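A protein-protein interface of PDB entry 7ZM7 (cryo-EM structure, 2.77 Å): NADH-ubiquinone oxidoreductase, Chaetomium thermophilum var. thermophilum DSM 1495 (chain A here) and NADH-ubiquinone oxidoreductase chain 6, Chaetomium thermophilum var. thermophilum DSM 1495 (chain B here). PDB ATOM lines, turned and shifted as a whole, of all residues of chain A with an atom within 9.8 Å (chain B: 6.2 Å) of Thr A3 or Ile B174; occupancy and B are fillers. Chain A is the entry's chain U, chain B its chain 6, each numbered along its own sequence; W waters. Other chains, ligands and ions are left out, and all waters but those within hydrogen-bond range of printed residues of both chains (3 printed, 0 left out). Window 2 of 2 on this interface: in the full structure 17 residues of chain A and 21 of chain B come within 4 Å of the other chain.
The backbone NH of Ala A2 sits at hydrogen-bond distance from the backbone carbonyl oxygen of Ile B170, 3.4 Å away.
N of Ser B172 is in hydrogen-bond range of O of Ala A2 (2.9 Å).
Met A1 touches Ile B170.
Met A1 touches Thr B171 (CB to C, 3.3 Å).
Met A1 touches Ser B172 (CB to N, 3.5 Å).
O of Ala A2 touches CA of Thr B171, at 3.3 Å.
Ser B172 touches Thr A3 (O to CA, 3.9 Å).
Thr A3 touches Ile B174.
Arg A4 touches Thr B171 (NH1 to CG2, 3.1 Å).
Pro A6 touches Thr B171.
Of chain B, only Ser B172 (3.9 Å) and Ile B174 (3.8 Å) come within 4 Å of Thr A3.
Of chain A, only Thr A3 (3.8 Å) comes within 4 Å of Ile B174.
No residue of chain A comes within 4 Å of Trp B175.
Printed residues of chain B within 4 Å of Pro A6: Thr B171 (3.8 Å).
Of the printed residues of chain B, Ala A2 touches Ile B170 (3.4 Å), Thr B171 (3.3 Å) and Ser B172 (2.9 Å).
Of the printed residues of chain A, Ser B172 touches Met A1 (3.5 Å), Ala A2 (2.9 Å) and Thr A3 (3.9 Å).
Of the printed residues of chain A, Thr B171 touches Met A1, Ala A2, Arg A4 and Pro A6.
Lys A5 touches none of the printed residues of chain B.
Asp B176 touches none of the printed residues of chain A.
The nearest residue of chain B that does not touch Thr A3 is Thr B171 (5.0 Å).
The nearest residue of chain A that does not touch Ile B174 is Ala A2 (6.9 Å).
The nearest printed residue of chain A that does not touch Thr B171 is Thr A3 (5.0 Å).
Printed residues of chain A that touch a printed residue of chain B: Met A1, Ala A2, Thr A3, Arg A4 and Pro A6.
Of the 9 printed residues of chain B, 4 touch a printed residue of chain A.
Hydrophobic or aromatic side chains of chain B within 4 Å of the printed part of chain A: Ile B170 and Ile B174.
Among the printed residues, 10 pairs touch across the chains.
Among the printed residues, no Asp or Glu carboxylate lies within 4 Å of a Lys or Arg side-chain nitrogen of the other chain.
Water W2 lies within hydrogen-bond range of the side-chain hydroxyl of Thr B171 (2.7 Å) and the guanidinium group of Arg A4 (3.4 Å).
Water W3 bridges NH1 of Arg A4 (3.1 Å) and O of Ile B170 (3.2 Å).
Water W1 lies within hydrogen-bond range of the side-chain carboxylate of Asp B176 and the side-chain carboxylate of Glu A66.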
ATOM      1  N   MET A   1       4.738 -25.809 -19.086  1.00  0.00           N
ATOM      2  CA  MET A   1       6.115 -25.370 -19.206  1.00  0.00           C
ATOM      3  C   MET A   1       6.152 -23.940 -19.685  1.00  0.00           C
ATOM      4  O   MET A   1       5.142 -23.425 -20.146  1.00  0.00           O
ATOM      5  CB  MET A   1       6.861 -26.276 -20.155  1.00  0.00           C
ATOM      6  N   ALA A   2       7.326 -23.316 -19.585  1.00  0.00           N
ATOM      7  CA  ALA A   2       7.432 -21.860 -19.827  1.00  0.00           C
ATOM      8  C   ALA A   2       6.940 -21.494 -21.222  1.00  0.00           C
ATOM      9  O   ALA A   2       7.005 -22.345 -22.108  1.00  0.00           O
ATOM     10  CB  ALA A   2       8.862 -21.439 -19.621  1.00  0.00           C
ATOM     11  N   THR A   3       6.519 -20.243 -21.416  1.00  0.00           N
ATOM     12  CA  THR A   3       5.945 -19.825 -22.724  1.00  0.00           C
ATOM     13  C   THR A   3       7.038 -19.259 -23.630  1.00  0.00           C
ATOM     14  O   THR A   3       6.702 -18.784 -24.719  1.00  0.00           O
ATOM     15  CB  THR A   3       4.811 -18.814 -22.533  1.00  0.00           C
ATOM     16  OG1 THR A   3       5.296 -17.769 -21.688  1.00  0.00           O
ATOM     17  CG2 THR A   3       3.567 -19.419 -21.930  1.00  0.00           C
ATOM     18  N   ARG A   4       8.287 -19.284 -23.183  1.00  0.00           N
ATOM     19  CA  ARG A   4       9.428 -18.728 -23.952  1.00  0.00           C
ATOM     20  C   ARG A   4       9.630 -19.489 -25.256  1.00  0.00           C
ATOM     21  O   ARG A   4       9.530 -20.715 -25.234  1.00  0.00           O
ATOM     22  CB  ARG A   4      10.693 -18.878 -23.111  1.00  0.00           C
ATOM     23  CG  ARG A   4      11.952 -18.358 -23.781  1.00  0.00           C
ATOM     24  CD  ARG A   4      13.154 -18.796 -22.981  1.00  0.00           C
ATOM     25  NE  ARG A   4      13.042 -20.157 -22.475  1.00  0.00           N
ATOM     26  CZ  ARG A   4      13.526 -21.236 -23.078  1.00  0.00           C
ATOM     27  NH1 ARG A   4      13.376 -22.425 -22.523  1.00  0.00           N
ATOM     28  NH2 ARG A   4      14.163 -21.123 -24.228  1.00  0.00           N
ATOM     29  N   LYS A   5       9.916 -18.775 -26.349  1.00  0.00           N
ATOM     30  CA  LYS A   5      10.238 -19.445 -27.631  1.00  0.00           C
ATOM     31  C   LYS A   5      11.564 -20.209 -27.454  1.00  0.00           C
ATOM     32  O   LYS A   5      12.478 -19.622 -26.851  1.00  0.00           O
ATOM     33  CB  LYS A   5      10.371 -18.402 -28.734  1.00  0.00           C
ATOM     34  CG  LYS A   5       9.154 -17.521 -28.968  1.00  0.00           C
ATOM     35  CD  LYS A   5       9.301 -16.646 -30.195  1.00  0.00           C
ATOM     36  CE  LYS A   5      10.633 -15.930 -30.248  1.00  0.00           C
ATOM     37  NZ  LYS A   5      10.773 -15.111 -31.475  1.00  0.00           N
ATOM     38  N   PRO A   6      11.730 -21.484 -27.895  1.00  0.00           N
ATOM     39  CA  PRO A   6      12.979 -22.193 -27.665  1.00  0.00           C
ATOM     40  C   PRO A   6      14.025 -21.985 -28.772  1.00  0.00           C
ATOM     41  O   PRO A   6      13.642 -21.863 -29.912  1.00  0.00           O
ATOM     42  CB  PRO A   6      12.486 -23.634 -27.537  1.00  0.00           C
ATOM     43  CG  PRO A   6      11.292 -23.719 -28.460  1.00  0.00           C
ATOM     44  CD  PRO A   6      10.711 -22.323 -28.521  1.00  0.00           C
ATOM     45  N   MET A  55     -13.254 -17.593 -20.833  1.00  0.00           N
ATOM     46  CA  MET A  55     -12.149 -16.611 -20.776  1.00  0.00           C
ATOM     47  C   MET A  55     -12.440 -15.679 -19.620  1.00  0.00           C
ATOM     48  O   MET A  55     -11.494 -15.175 -19.023  1.00  0.00           O
ATOM     49  CB  MET A  55     -12.080 -15.832 -22.093  1.00  0.00           C
ATOM     50  CG  MET A  55     -11.659 -16.696 -23.257  1.00  0.00           C
ATOM     51  SD  MET A  55     -10.004 -17.376 -23.044  1.00  0.00           S
ATOM     52  CE  MET A  55      -9.016 -15.903 -23.289  1.00  0.00           C
ATOM     53  N   LYS A  58     -11.460 -17.488 -16.236  1.00  0.00           N
ATOM     54  CA  LYS A  58      -9.987 -17.449 -16.048  1.00  0.00           C
ATOM     55  C   LYS A  58      -9.568 -16.058 -15.585  1.00  0.00           C
ATOM     56  O   LYS A  58      -8.714 -15.973 -14.701  1.00  0.00           O
ATOM     57  CB  LYS A  58      -9.291 -17.794 -17.364  1.00  0.00           C
ATOM     58  CG  LYS A  58      -9.431 -19.231 -17.838  1.00  0.00           C
ATOM     59  CD  LYS A  58      -8.693 -19.477 -19.129  1.00  0.00           C
ATOM     60  CE  LYS A  58      -7.197 -19.283 -19.007  1.00  0.00           C
ATOM     61  NZ  LYS A  58      -6.604 -20.211 -18.018  1.00  0.00           N
ATOM     62  N   GLU A  66      -5.960 -22.188 -14.612  1.00  0.00           N
ATOM     63  CA  GLU A  66      -5.904 -23.460 -15.366  1.00  0.00           C
ATOM     64  C   GLU A  66      -6.746 -24.420 -14.529  1.00  0.00           C
ATOM     65  O   GLU A  66      -7.601 -25.091 -15.096  1.00  0.00           O
ATOM     66  CB  GLU A  66      -4.435 -23.860 -15.534  1.00  0.00           C
ATOM     67  CG  GLU A  66      -3.661 -22.974 -16.492  1.00  0.00           C
ATOM     68  CD  GLU A  66      -3.406 -21.540 -16.055  1.00  0.00           C
ATOM     69  OE1 GLU A  66      -3.355 -21.286 -14.831  1.00  0.00           O
ATOM     70  OE2 GLU A  66      -3.270 -20.674 -16.943  1.00  0.00           O
ATOM     71  N   ILE B 170      12.404 -26.342 -19.699  1.00  0.00           N
ATOM     72  CA  ILE B 170      11.233 -26.933 -20.408  1.00  0.00           C
ATOM     73  C   ILE B 170      10.374 -25.804 -20.974  1.00  0.00           C
ATOM     74  O   ILE B 170      10.272 -24.763 -20.308  1.00  0.00           O
ATOM     75  CB  ILE B 170      10.439 -27.891 -19.489  1.00  0.00           C
ATOM     76  CG1 ILE B 170       9.353 -28.662 -20.244  1.00  0.00           C
ATOM     77  CG2 ILE B 170       9.884 -27.179 -18.266  1.00  0.00           C
ATOM     78  CD1 ILE B 170       9.761 -30.048 -20.655  1.00  0.00           C
ATOM     79  N   THR B 171       9.822 -25.990 -22.174  1.00  0.00           N
ATOM     80  CA  THR B 171       8.896 -24.981 -22.748  1.00  0.00           C
ATOM     81  C   THR B 171       7.641 -25.651 -23.313  1.00  0.00           C
ATOM     82  O   THR B 171       7.741 -26.807 -23.737  1.00  0.00           O
ATOM     83  CB  THR B 171       9.572 -24.084 -23.790  1.00  0.00           C
ATOM     84  OG1 THR B 171      10.396 -24.882 -24.640  1.00  0.00           O
ATOM     85  CG2 THR B 171      10.370 -22.961 -23.167  1.00  0.00           C
ATOM     86  N   SER B 172       6.515 -24.935 -23.322  1.00  0.00           N
ATOM     87  CA  SER B 172       5.228 -25.452 -23.855  1.00  0.00           C
ATOM     88  C   SER B 172       4.539 -24.316 -24.612  1.00  0.00           C
ATOM     89  O   SER B 172       4.977 -23.166 -24.451  1.00  0.00           O
ATOM     90  CB  SER B 172       4.364 -25.974 -22.751  1.00  0.00           C
ATOM     91  OG  SER B 172       3.071 -26.302 -23.225  1.00  0.00           O
ATOM     92  N   LYS B 173       3.514 -24.622 -25.412  1.00  0.00           N
ATOM     93  CA  LYS B 173       2.842 -23.597 -26.253  1.00  0.00           C
ATOM     94  C   LYS B 173       1.759 -22.833 -25.485  1.00  0.00           C
ATOM     95  O   LYS B 173       1.330 -23.328 -24.433  1.00  0.00           O
ATOM     96  CB  LYS B 173       2.263 -24.273 -27.498  1.00  0.00           C
ATOM     97  CG  LYS B 173       1.322 -25.439 -27.248  1.00  0.00           C
ATOM     98  CD  LYS B 173       0.844 -26.114 -28.513  1.00  0.00           C
ATOM     99  CE  LYS B 173       1.960 -26.756 -29.310  1.00  0.00           C
ATOM    100  NZ  LYS B 173       1.437 -27.474 -30.496  1.00  0.00           N
ATOM    101  N   ILE B 174       1.359 -21.659 -25.983  1.00  0.00           N
ATOM    102  CA  ILE B 174       0.253 -20.847 -25.389  1.00  0.00           C
ATOM    103  C   ILE B 174      -0.561 -20.353 -26.585  1.00  0.00           C
ATOM    104  O   ILE B 174       0.011 -20.273 -27.674  1.00  0.00           O
ATOM    105  CB  ILE B 174       0.808 -19.670 -24.557  1.00  0.00           C
ATOM    106  CG1 ILE B 174      -0.231 -19.064 -23.615  1.00  0.00           C
ATOM    107  CG2 ILE B 174       1.444 -18.612 -25.445  1.00  0.00           C
ATOM    108  CD1 ILE B 174       0.236 -17.792 -22.953  1.00  0.00           C
ATOM    109  N   TRP B 175      -1.852 -20.089 -26.410  1.00  0.00           N
ATOM    110  CA  TRP B 175      -2.690 -19.710 -27.571  1.00  0.00           C
ATOM    111  C   TRP B 175      -3.208 -18.282 -27.429  1.00  0.00           C
ATOM    112  O   TRP B 175      -3.148 -17.534 -28.409  1.00  0.00           O
ATOM    113  CB  TRP B 175      -3.805 -20.735 -27.753  1.00  0.00           C
ATOM    114  CG  TRP B 175      -3.288 -22.089 -28.127  1.00  0.00           C
ATOM    115  CD1 TRP B 175      -3.113 -23.163 -27.303  1.00  0.00           C
ATOM    116  CD2 TRP B 175      -2.844 -22.509 -29.428  1.00  0.00           C
ATOM    117  NE1 TRP B 175      -2.613 -24.224 -28.005  1.00  0.00           N
ATOM    118  CE2 TRP B 175      -2.435 -23.853 -29.310  1.00  0.00           C
ATOM    119  CE3 TRP B 175      -2.758 -21.885 -30.678  1.00  0.00           C
ATOM    120  CZ2 TRP B 175      -1.952 -24.581 -30.395  1.00  0.00           C
ATOM    121  CZ3 TRP B 175      -2.284 -22.605 -31.748  1.00  0.00           C
ATOM    122  CH2 TRP B 175      -1.892 -23.935 -31.607  1.00  0.00           C
ATOM    123  N   ASP B 176      -3.668 -17.913 -26.241  1.00  0.00           N
ATOM    124  CA  ASP B 176      -4.150 -16.532 -25.977  1.00  0.00           C
ATOM    125  C   ASP B 176      -3.001 -15.535 -26.159  1.00  0.00           C
ATOM    126  O   ASP B 176      -3.268 -14.432 -26.664  1.00  0.00           O
ATOM    127  CB  ASP B 176      -4.901 -16.424 -24.644  1.00  0.00           C
ATOM    128  CG  ASP B 176      -4.289 -17.175 -23.473  1.00  0.00           C
ATOM    129  OD1 ASP B 176      -3.082 -17.467 -23.523  1.00  0.00           O
ATOM    130  OD2 ASP B 176      -5.031 -17.451 -22.512  1.00  0.00           O
ATOM    131  N   GLY B 177      -1.782 -15.910 -25.766  1.00  0.00           N
ATOM    132  CA  GLY B 177      -0.601 -15.036 -25.890  1.00  0.00           C
ATOM    133  C   GLY B 177       0.079 -15.121 -27.246  1.00  0.00           C
ATOM    134  O   GLY B 177       1.063 -14.400 -27.442  1.00  0.00           O
ATOM    135  N   ALA B 178      -0.411 -15.973 -28.148  1.00  0.00           N
ATOM    136  CA  ALA B 178       0.185 -16.134 -29.495  1.00  0.00           C
ATOM    137  C   ALA B 178      -0.760 -15.618 -30.581  1.00  0.00           C
ATOM    138  O   ALA B 178      -0.537 -15.965 -31.733  1.00  0.00           O
ATOM    139  CB  ALA B 178       0.525 -17.583 -29.728  1.00  0.00           C
HETATM  140  O   HOH W   1      -3.349 -19.064 -20.016  1.00  0.00           O
HETATM  141  O   HOH W   2      12.972 -25.462 -23.954  1.00  0.00           O
HETATM  142  O   HOH W   3      12.302 -22.379 -19.594  1.00  0.00           O
